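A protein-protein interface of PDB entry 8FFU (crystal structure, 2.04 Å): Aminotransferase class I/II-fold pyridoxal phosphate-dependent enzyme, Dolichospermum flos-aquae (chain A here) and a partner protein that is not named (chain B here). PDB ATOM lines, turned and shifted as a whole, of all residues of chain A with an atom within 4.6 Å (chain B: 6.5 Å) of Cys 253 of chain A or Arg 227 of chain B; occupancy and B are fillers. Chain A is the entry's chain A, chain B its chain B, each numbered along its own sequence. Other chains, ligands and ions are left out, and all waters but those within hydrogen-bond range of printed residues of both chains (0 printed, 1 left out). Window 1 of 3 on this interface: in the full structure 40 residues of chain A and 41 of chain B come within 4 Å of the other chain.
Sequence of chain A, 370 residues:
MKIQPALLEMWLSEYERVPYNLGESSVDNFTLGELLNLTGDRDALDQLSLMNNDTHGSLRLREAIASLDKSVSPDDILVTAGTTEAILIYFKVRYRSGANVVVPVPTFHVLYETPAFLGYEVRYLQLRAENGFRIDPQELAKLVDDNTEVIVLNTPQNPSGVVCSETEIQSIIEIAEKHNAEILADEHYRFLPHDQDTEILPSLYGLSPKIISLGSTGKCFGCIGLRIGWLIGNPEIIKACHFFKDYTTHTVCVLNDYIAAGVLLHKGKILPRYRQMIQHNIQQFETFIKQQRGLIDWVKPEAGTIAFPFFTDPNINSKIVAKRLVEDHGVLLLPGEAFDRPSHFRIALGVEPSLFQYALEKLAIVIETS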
ATOM      1  N   ASN A  53      -1.328  10.399 -35.003  1.00  0.00           N
ATOM      2  CA  ASN A  53      -1.373  11.586 -35.842  1.00  0.00           C
ATOM      3  C   ASN A  53      -0.036  12.319 -35.762  1.00  0.00           C
ATOM      4  O   ASN A  53       0.803  12.047 -34.898  1.00  0.00           O
ATOM      5  CB  ASN A  53      -2.522  12.490 -35.382  1.00  0.00           C
ATOM      6  CG  ASN A  53      -2.799  13.645 -36.326  1.00  0.00           C
ATOM      7  OD1 ASN A  53      -2.467  13.602 -37.509  1.00  0.00           O
ATOM      8  ND2 ASN A  53      -3.425  14.688 -35.800  1.00  0.00           N
ATOM      9  N   THR A 249      -1.639  14.485 -23.526  1.00  0.00           N
ATOM     10  CA  THR A 249      -2.388  13.554 -24.364  1.00  0.00           C
ATOM     11  C   THR A 249      -1.580  13.034 -25.542  1.00  0.00           C
ATOM     12  O   THR A 249      -2.087  12.183 -26.286  1.00  0.00           O
ATOM     13  CB  THR A 249      -3.675  14.200 -24.915  1.00  0.00           C
ATOM     14  OG1 THR A 249      -3.337  15.264 -25.815  1.00  0.00           O
ATOM     15  CG2 THR A 249      -4.554  14.740 -23.791  1.00  0.00           C
ATOM     16  N   HIS A 250      -0.359  13.535 -25.744  1.00  0.00           N
ATOM     17  CA  HIS A 250       0.540  13.147 -26.824  1.00  0.00           C
ATOM     18  C   HIS A 250       0.024  13.599 -28.191  1.00  0.00           C
ATOM     19  O   HIS A 250       0.656  14.444 -28.833  1.00  0.00           O
ATOM     20  CB  HIS A 250       0.801  11.636 -26.787  1.00  0.00           C
ATOM     21  CG  HIS A 250       1.837  11.181 -27.763  1.00  0.00           C
ATOM     22  ND1 HIS A 250       1.578  10.259 -28.751  1.00  0.00           N
ATOM     23  CD2 HIS A 250       3.132  11.548 -27.919  1.00  0.00           C
ATOM     24  CE1 HIS A 250       2.670  10.066 -29.468  1.00  0.00           C
ATOM     25  NE2 HIS A 250       3.628  10.836 -28.984  1.00  0.00           N
ATOM     26  N   THR A 251      -1.104  13.056 -28.657  1.00  0.00           N
ATOM     27  CA  THR A 251      -1.674  13.443 -29.946  1.00  0.00           C
ATOM     28  C   THR A 251      -3.190  13.538 -29.826  1.00  0.00           C
ATOM     29  O   THR A 251      -3.782  13.077 -28.848  1.00  0.00           O
ATOM     30  CB  THR A 251      -1.325  12.451 -31.080  1.00  0.00           C
ATOM     31  OG1 THR A 251      -1.788  11.135 -30.748  1.00  0.00           O
ATOM     32  CG2 THR A 251       0.170  12.405 -31.339  1.00  0.00           C
ATOM     33  N   VAL A 252      -3.813  14.177 -30.821  1.00  0.00           N
ATOM     34  CA  VAL A 252      -5.257  14.105 -31.013  1.00  0.00           C
ATOM     35  C   VAL A 252      -5.530  13.153 -32.169  1.00  0.00           C
ATOM     36  O   VAL A 252      -4.676  12.907 -33.024  1.00  0.00           O
ATOM     37  CB  VAL A 252      -5.918  15.484 -31.275  1.00  0.00           C
ATOM     38  CG1 VAL A 252      -5.619  16.462 -30.152  1.00  0.00           C
ATOM     39  CG2 VAL A 252      -5.496  16.034 -32.629  1.00  0.00           C
ATOM     40  N   CYS A 253      -6.741  12.610 -32.202  1.00  0.00           N
ATOM     41  CA  CYS A 253      -7.083  11.620 -33.215  1.00  0.00           C
ATOM     42  C   CYS A 253      -7.096  12.232 -34.613  1.00  0.00           C
ATOM     43  O   CYS A 253      -7.534  13.370 -34.809  1.00  0.00           O
ATOM     44  CB  CYS A 253      -8.437  10.992 -32.912  1.00  0.00           C
ATOM     45  SG  CYS A 253      -8.824   9.627 -34.011  1.00  0.00           S
ATOM     46  N   VAL A 254      -6.620  11.456 -35.589  1.00  0.00           N
ATOM     47  CA  VAL A 254      -6.604  11.899 -36.982  1.00  0.00           C
ATOM     48  C   VAL A 254      -8.009  12.193 -37.504  1.00  0.00           C
ATOM     49  O   VAL A 254      -8.171  12.979 -38.443  1.00  0.00           O
ATOM     50  CB  VAL A 254      -5.881  10.848 -37.850  1.00  0.00           C
ATOM     51  CG1 VAL A 254      -6.653   9.539 -37.856  1.00  0.00           C
ATOM     52  CG2 VAL A 254      -5.655  11.367 -39.270  1.00  0.00           C
ATOM     53  N   LEU A 255      -9.041  11.559 -36.938  1.00  0.00           N
ATOM     54  CA  LEU A 255     -10.404  11.825 -37.396  1.00  0.00           C
ATOM     55  C   LEU A 255     -10.892  13.186 -36.921  1.00  0.00           C
ATOM     56  O   LEU A 255     -11.397  13.982 -37.719  1.00  0.00           O
ATOM     57  CB  LEU A 255     -11.375  10.736 -36.945  1.00  0.00           C
ATOM     58  CG  LEU A 255     -11.240   9.336 -37.534  1.00  0.00           C
ATOM     59  CD1 LEU A 255     -11.161   9.440 -39.043  1.00  0.00           C
ATOM     60  CD2 LEU A 255     -10.057   8.581 -36.986  1.00  0.00           C
ATOM     61  N   ASN A 256     -10.774  13.457 -35.619  1.00  0.00           N
ATOM     62  CA  ASN A 256     -11.168  14.756 -35.087  1.00  0.00           C
ATOM     63  C   ASN A 256     -10.413  15.866 -35.801  1.00  0.00           C
ATOM     64  O   ASN A 256     -10.990  16.885 -36.197  1.00  0.00           O
ATOM     65  CB  ASN A 256     -10.861  14.817 -33.590  1.00  0.00           C
ATOM     66  CG  ASN A 256     -11.516  13.705 -32.805  1.00  0.00           C
ATOM     67  OD1 ASN A 256     -11.739  12.613 -33.323  1.00  0.00           O
ATOM     68  ND2 ASN A 256     -11.807  13.970 -31.538  1.00  0.00           N
ATOM     69  N   ASP A 257      -9.105  15.675 -35.956  1.00  0.00           N
ATOM     70  CA  ASP A 257      -8.268  16.592 -36.712  1.00  0.00           C
ATOM     71  C   ASP A 257      -8.814  16.798 -38.119  1.00  0.00           C
ATOM     72  O   ASP A 257      -9.028  17.932 -38.560  1.00  0.00           O
ATOM     73  CB  ASP A 257      -6.841  16.032 -36.733  1.00  0.00           C
ATOM     74  CG  ASP A 257      -5.852  16.943 -37.410  1.00  0.00           C
ATOM     75  OD1 ASP A 257      -6.035  17.268 -38.599  1.00  0.00           O
ATOM     76  OD2 ASP A 257      -4.874  17.330 -36.745  1.00  0.00           O
ATOM     77  N   VAL B  79     -13.131   7.601 -18.246  1.00  0.00           N
ATOM     78  CA  VAL B  79     -12.511   7.540 -19.564  1.00  0.00           C
ATOM     79  C   VAL B  79     -11.682   8.793 -19.807  1.00  0.00           C
ATOM     80  O   VAL B  79     -12.118   9.914 -19.517  1.00  0.00           O
ATOM     81  CB  VAL B  79     -13.594   7.365 -20.642  1.00  0.00           C
ATOM     82  CG1 VAL B  79     -12.984   7.370 -22.035  1.00  0.00           C
ATOM     83  CG2 VAL B  79     -14.369   6.084 -20.398  1.00  0.00           C
ATOM     84  N   THR B  80     -10.481   8.609 -20.357  1.00  0.00           N
ATOM     85  CA  THR B  80      -9.529   9.689 -20.579  1.00  0.00           C
ATOM     86  C   THR B  80      -8.982   9.626 -22.002  1.00  0.00           C
ATOM     87  O   THR B  80      -9.232   8.679 -22.753  1.00  0.00           O
ATOM     88  CB  THR B  80      -8.367   9.635 -19.572  1.00  0.00           C
ATOM     89  OG1 THR B  80      -7.675   8.384 -19.696  1.00  0.00           O
ATOM     90  CG2 THR B  80      -8.874   9.791 -18.140  1.00  0.00           C
ATOM     91  N   ALA B  81      -8.232  10.669 -22.370  1.00  0.00           N
ATOM     92  CA  ALA B  81      -7.598  10.769 -23.687  1.00  0.00           C
ATOM     93  C   ALA B  81      -6.253  10.053 -23.634  1.00  0.00           C
ATOM     94  O   ALA B  81      -5.191  10.660 -23.491  1.00  0.00           O
ATOM     95  CB  ALA B  81      -7.444  12.225 -24.102  1.00  0.00           C
ATOM     96  N   GLY B  82      -6.309   8.735 -23.764  1.00  0.00           N
ATOM     97  CA  GLY B  82      -5.159   7.895 -23.514  1.00  0.00           C
ATOM     98  C   GLY B  82      -4.876   7.777 -22.028  1.00  0.00           C
ATOM     99  O   GLY B  82      -5.396   8.519 -21.201  1.00  0.00           O
ATOM    100  N   THR B  83      -4.045   6.801 -21.681  1.00  0.00           N
ATOM    101  CA  THR B  83      -3.617   6.714 -20.291  1.00  0.00           C
ATOM    102  C   THR B  83      -2.631   7.815 -19.940  1.00  0.00           C
ATOM    103  O   THR B  83      -2.398   8.060 -18.753  1.00  0.00           O
ATOM    104  CB  THR B  83      -3.005   5.337 -19.998  1.00  0.00           C
ATOM    105  OG1 THR B  83      -1.812   5.174 -20.767  1.00  0.00           O
ATOM    106  CG2 THR B  83      -3.983   4.234 -20.363  1.00  0.00           C
ATOM    107  N   THR B  84      -2.070   8.497 -20.941  1.00  0.00           N
ATOM    108  CA  THR B  84      -1.199   9.634 -20.667  1.00  0.00           C
ATOM    109  C   THR B  84      -1.930  10.694 -19.852  1.00  0.00           C
ATOM    110  O   THR B  84      -1.379  11.236 -18.886  1.00  0.00           O
ATOM    111  CB  THR B  84      -0.685  10.236 -21.979  1.00  0.00           C
ATOM    112  OG1 THR B  84      -0.012   9.232 -22.747  1.00  0.00           O
ATOM    113  CG2 THR B  84       0.270  11.379 -21.704  1.00  0.00           C
ATOM    114  N   GLU B  85      -3.185  10.982 -20.213  1.00  0.00           N
ATOM    115  CA  GLU B  85      -3.993  11.924 -19.446  1.00  0.00           C
ATOM    116  C   GLU B  85      -4.346  11.355 -18.081  1.00  0.00           C
ATOM    117  O   GLU B  85      -4.343  12.082 -17.081  1.00  0.00           O
ATOM    118  CB  GLU B  85      -5.258  12.285 -20.225  1.00  0.00           C
ATOM    119  CG  GLU B  85      -6.128  13.329 -19.547  1.00  0.00           C
ATOM    120  CD  GLU B  85      -7.417  13.615 -20.299  1.00  0.00           C
ATOM    121  OE1 GLU B  85      -8.002  12.689 -20.896  1.00  0.00           O
ATOM    122  OE2 GLU B  85      -7.844  14.785 -20.299  1.00  0.00           O
ATOM    123  N   SER B 216      -6.467   0.659 -21.689  1.00  0.00           N
ATOM    124  CA  SER B 216      -6.645   1.343 -22.964  1.00  0.00           C
ATOM    125  C   SER B 216      -6.790   0.319 -24.079  1.00  0.00           C
ATOM    126  O   SER B 216      -6.293  -0.806 -23.975  1.00  0.00           O
ATOM    127  CB  SER B 216      -5.474   2.286 -23.271  1.00  0.00           C
ATOM    128  OG  SER B 216      -5.610   2.864 -24.560  1.00  0.00           O
ATOM    129  N   GLY B 218      -5.685   1.244 -27.098  1.00  0.00           N
ATOM    130  CA  GLY B 218      -4.785   1.769 -28.110  1.00  0.00           C
ATOM    131  C   GLY B 218      -3.720   0.853 -28.674  1.00  0.00           C
ATOM    132  O   GLY B 218      -3.666   0.637 -29.881  1.00  0.00           O
ATOM    133  N1  LLP B 219       2.100   3.105 -20.632  1.00  0.00           N
ATOM    134  C2  LLP B 219       2.531   2.130 -21.437  1.00  0.00           C
ATOM    135  C2' LLP B 219       3.190   0.944 -20.800  1.00  0.00           C
ATOM    136  C3  LLP B 219       2.371   2.205 -22.826  1.00  0.00           C
ATOM    137  O3  LLP B 219       2.835   1.167 -23.562  1.00  0.00           O
ATOM    138  C4  LLP B 219       1.745   3.329 -23.395  1.00  0.00           C
ATOM    139  C4' LLP B 219       1.575   3.409 -24.846  1.00  0.00           C
ATOM    140  C5  LLP B 219       1.295   4.352 -22.529  1.00  0.00           C
ATOM    141  C6  LLP B 219       1.502   4.169 -21.178  1.00  0.00           C
ATOM    142  C5' LLP B 219       0.629   5.616 -23.007  1.00  0.00           C
ATOM    143  OP4 LLP B 219      -0.083   5.554 -24.252  1.00  0.00           O
ATOM    144  P   LLP B 219      -1.598   6.021 -24.292  1.00  0.00           P
ATOM    145  OP1 LLP B 219      -1.692   7.453 -23.898  1.00  0.00           O
ATOM    146  OP2 LLP B 219      -2.369   5.101 -23.346  1.00  0.00           O
ATOM    147  OP3 LLP B 219      -2.069   5.731 -25.706  1.00  0.00           O
ATOM    148  N   LLP B 219      -2.873   0.314 -27.804  1.00  0.00           N
ATOM    149  CA  LLP B 219      -1.687  -0.438 -28.246  1.00  0.00           C
ATOM    150  CB  LLP B 219      -0.644  -0.434 -27.124  1.00  0.00           C
ATOM    151  CG  LLP B 219      -0.120   0.955 -26.753  1.00  0.00           C
ATOM    152  CD  LLP B 219       0.978   1.500 -27.664  1.00  0.00           C
ATOM    153  CE  LLP B 219       1.700   2.717 -27.086  1.00  0.00           C
ATOM    154  NZ  LLP B 219       1.958   2.517 -25.663  1.00  0.00           N
ATOM    155  C   LLP B 219      -2.010  -1.867 -28.671  1.00  0.00           C
ATOM    156  O   LLP B 219      -1.298  -2.450 -29.464  1.00  0.00           O
ATOM    157  N   CYS B 223      -5.384   0.669 -32.816  1.00  0.00           N
ATOM    158  CA  CYS B 223      -6.033   1.969 -32.937  1.00  0.00           C
ATOM    159  C   CYS B 223      -5.454   2.940 -31.910  1.00  0.00           C
ATOM    160  O   CYS B 223      -6.178   3.584 -31.151  1.00  0.00           O
ATOM    161  CB  CYS B 223      -7.547   1.829 -32.782  1.00  0.00           C
ATOM    162  SG  CYS B 223      -8.050   1.022 -31.252  1.00  0.00           S
ATOM    163  N   ILE B 224      -4.125   3.065 -31.884  1.00  0.00           N
ATOM    164  CA  ILE B 224      -3.475   3.919 -30.891  1.00  0.00           C
ATOM    165  C   ILE B 224      -3.926   5.369 -31.048  1.00  0.00           C
ATOM    166  O   ILE B 224      -3.987   6.122 -30.066  1.00  0.00           O
ATOM    167  CB  ILE B 224      -1.940   3.773 -30.996  1.00  0.00           C
ATOM    168  CG1 ILE B 224      -1.225   4.599 -29.928  1.00  0.00           C
ATOM    169  CG2 ILE B 224      -1.442   4.177 -32.376  1.00  0.00           C
ATOM    170  CD1 ILE B 224      -1.647   4.271 -28.517  1.00  0.00           C
ATOM    171  N   GLY B 225      -4.277   5.773 -32.268  1.00  0.00           N
ATOM    172  CA  GLY B 225      -4.645   7.147 -32.551  1.00  0.00           C
ATOM    173  C   GLY B 225      -6.008   7.569 -32.041  1.00  0.00           C
ATOM    174  O   GLY B 225      -6.294   8.768 -32.054  1.00  0.00           O
ATOM    175  N   LEU B 226      -6.863   6.628 -31.623  1.00  0.00           N
ATOM    176  CA  LEU B 226      -8.170   7.020 -31.097  1.00  0.00           C
ATOM    177  C   LEU B 226      -8.059   7.871 -29.839  1.00  0.00           C
ATOM    178  O   LEU B 226      -8.953   8.678 -29.560  1.00  0.00           O
ATOM    179  CB  LEU B 226      -9.028   5.792 -30.805  1.00  0.00           C
ATOM    180  CG  LEU B 226      -9.679   5.107 -31.998  1.00  0.00           C
ATOM    181  CD1 LEU B 226     -10.563   3.976 -31.509  1.00  0.00           C
ATOM    182  CD2 LEU B 226     -10.495   6.108 -32.789  1.00  0.00           C
ATOM    183  N   ARG B 227      -6.967   7.723 -29.089  1.00  0.00           N
ATOM    184  CA  ARG B 227      -6.752   8.416 -27.817  1.00  0.00           C
ATOM    185  C   ARG B 227      -7.872   8.100 -26.822  1.00  0.00           C
ATOM    186  O   ARG B 227      -8.581   8.983 -26.338  1.00  0.00           O
ATOM    187  CB  ARG B 227      -6.616   9.931 -28.020  1.00  0.00           C
ATOM    188  CG  ARG B 227      -5.709  10.370 -29.168  1.00  0.00           C
ATOM    189  CD  ARG B 227      -4.285   9.838 -29.074  1.00  0.00           C
ATOM    190  NE  ARG B 227      -3.648  10.140 -27.802  1.00  0.00           N
ATOM    191  CZ  ARG B 227      -3.191   9.218 -26.964  1.00  0.00           C
ATOM    192  NH1 ARG B 227      -3.278   7.931 -27.245  1.00  0.00           N
ATOM    193  NH2 ARG B 227      -2.626   9.600 -25.822  1.00  0.00           N
ATOM    194  N   ILE B 228      -8.019   6.812 -26.515  1.00  0.00           N
ATOM    195  CA  ILE B 228      -8.999   6.357 -25.535  1.00  0.00           C
ATOM    196  C   ILE B 228      -8.291   5.480 -24.510  1.00  0.00           C
ATOM    197  O   ILE B 228      -7.694   4.458 -24.867  1.00  0.00           O
ATOM    198  CB  ILE B 228     -10.170   5.601 -26.185  1.00  0.00           C
ATOM    199  CG1 ILE B 228     -11.063   6.575 -26.954  1.00  0.00           C
ATOM    200  CG2 ILE B 228     -10.977   4.862 -25.125  1.00  0.00           C
ATOM    201  CD1 ILE B 228     -11.776   7.595 -26.067  1.00  0.00           C
ATOM    202  N   GLY B 229      -8.363   5.880 -23.245  1.00  0.00           N
ATOM    203  CA  GLY B 229      -7.887   5.101 -22.123  1.00  0.00           C
ATOM    204  C   GLY B 229      -8.876   5.226 -20.986  1.00  0.00           C
ATOM    205  O   GLY B 229      -9.941   5.812 -21.176  1.00  0.00           O
ATOM    206  N   VAL B 252     -13.459  13.635 -23.863  1.00  0.00           N
ATOM    207  CA  VAL B 252     -12.989  13.040 -25.098  1.00  0.00           C
ATOM    208  C   VAL B 252     -14.158  13.030 -26.073  1.00  0.00           C
ATOM    209  O   VAL B 252     -15.326  13.085 -25.679  1.00  0.00           O
ATOM    210  CB  VAL B 252     -12.423  11.613 -24.881  1.00  0.00           C
ATOM    211  CG1 VAL B 252     -11.307  11.638 -23.863  1.00  0.00           C
ATOM    212  CG2 VAL B 252     -13.524  10.659 -24.435  1.00  0.00           C
ATOM    213  N   ASN B 256     -14.717   9.032 -30.903  1.00  0.00           N
ATOM    214  CA  ASN B 256     -13.663   8.127 -30.451  1.00  0.00           C
ATOM    215  C   ASN B 256     -14.155   7.242 -29.317  1.00  0.00           C
ATOM    216  O   ASN B 256     -13.837   6.048 -29.264  1.00  0.00           O
ATOM    217  CB  ASN B 256     -12.437   8.923 -30.007  1.00  0.00           C
ATOM    218  CG  ASN B 256     -11.873   9.783 -31.114  1.00  0.00           C
ATOM    219  OD1 ASN B 256     -11.560   9.293 -32.197  1.00  0.00           O
ATOM    220  ND2 ASN B 256     -11.751  11.075 -30.854  1.00  0.00           N
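NH2 of Arg 227 of chain B sits at hydrogen-bond distance from O of Thr 249 of chain A (2.7 Å).
The backbone carbonyl oxygen of Thr 251 of chain A sits at hydrogen-bond distance from the guanidinium group of Arg 227 of chain B (3.1 Å).
The side-chain sulfur of Cys 253 of chain A sits close to the backbone carbonyl oxygen of Gly 225 of chain B (3.3 Å).
The side-chain sulfur (SG) of Cys 253 of chain A lies within hydrogen-bond range of the side-chain amide oxygen (OD1) of Asn 256 of chain B.
OD1 of Asn 256 of chain A sits at hydrogen-bond distance from ND2 of Asn 256 of chain B, at 2.9 Å.
The side-chain sulfur (SG) of Cys 253 of chain A sits close to the backbone NH (N) of Leu 255 of chain A (3.5 Å).
The backbone NH of Ala 81 of chain B lies within hydrogen-bond range of the side-chain carboxylate of Glu 85 of chain B, 2.5 Å away.
N of Gly 82 of chain B is in hydrogen-bond range of O of Arg 227 of chain B, 3.4 Å away.
OP3 of LLP 219 of chain B lies close to the guanidinium group (NH1) of Arg 227 of chain B.
O of Ile 224 of chain B is in hydrogen-bond range of NH1 of Arg 227 of chain B (3.4 Å).
Among the printed residues, merely in contact across the chains: Thr 249 of chain A with Ala 81 of chain B (3.8 Å), Cys 253 of chain A with Leu 226 of chain B (3.96 Å) and Cys 253 of chain A with Arg 227 of chain B (3.9 Å).
Of the printed residues of chain B, Thr 249 of chain A touches Ala 81 (3.8 Å) and Arg 227 (2.7 Å).
Printed residues of chain B within 4 Å of Thr 251 of chain A: Arg 227 (3.1 Å).
Of chain B, only Gly 225 (3.2 Å), Leu 226 (3.96 Å), Arg 227 (3.9 Å) and Asn 256 (3.3 Å) come within 4 Å of Cys 253 of chain A.
Printed residues of chain A within 4 Å of Gly 225 of chain B: Cys 253.
Printed residues of chain A within 4 Å of Leu 226 of chain B: Cys 253.
Of chain A, only Thr 249 (2.7 Å), Thr 251 (3.1 Å) and Cys 253 (3.9 Å) come within 4 Å of Arg 227 of chain B.
Gly 229 of chain B touches none of the printed residues of chain A.
The nearest printed residue of chain B that does not touch Cys 253 of chain A is Ile 224 of chain B (7.1 Å).
Of the 19 printed residues of chain B, 5 touch a printed residue of chain A.
Hydrophobic or aromatic side chains of chain B that line the printed part of chain A: Ala 81.
Along chain B the printed residues that touch a printed residue of chain A span positions 81 to 256.
Among the printed residues, 8 pairs touch across the chains.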
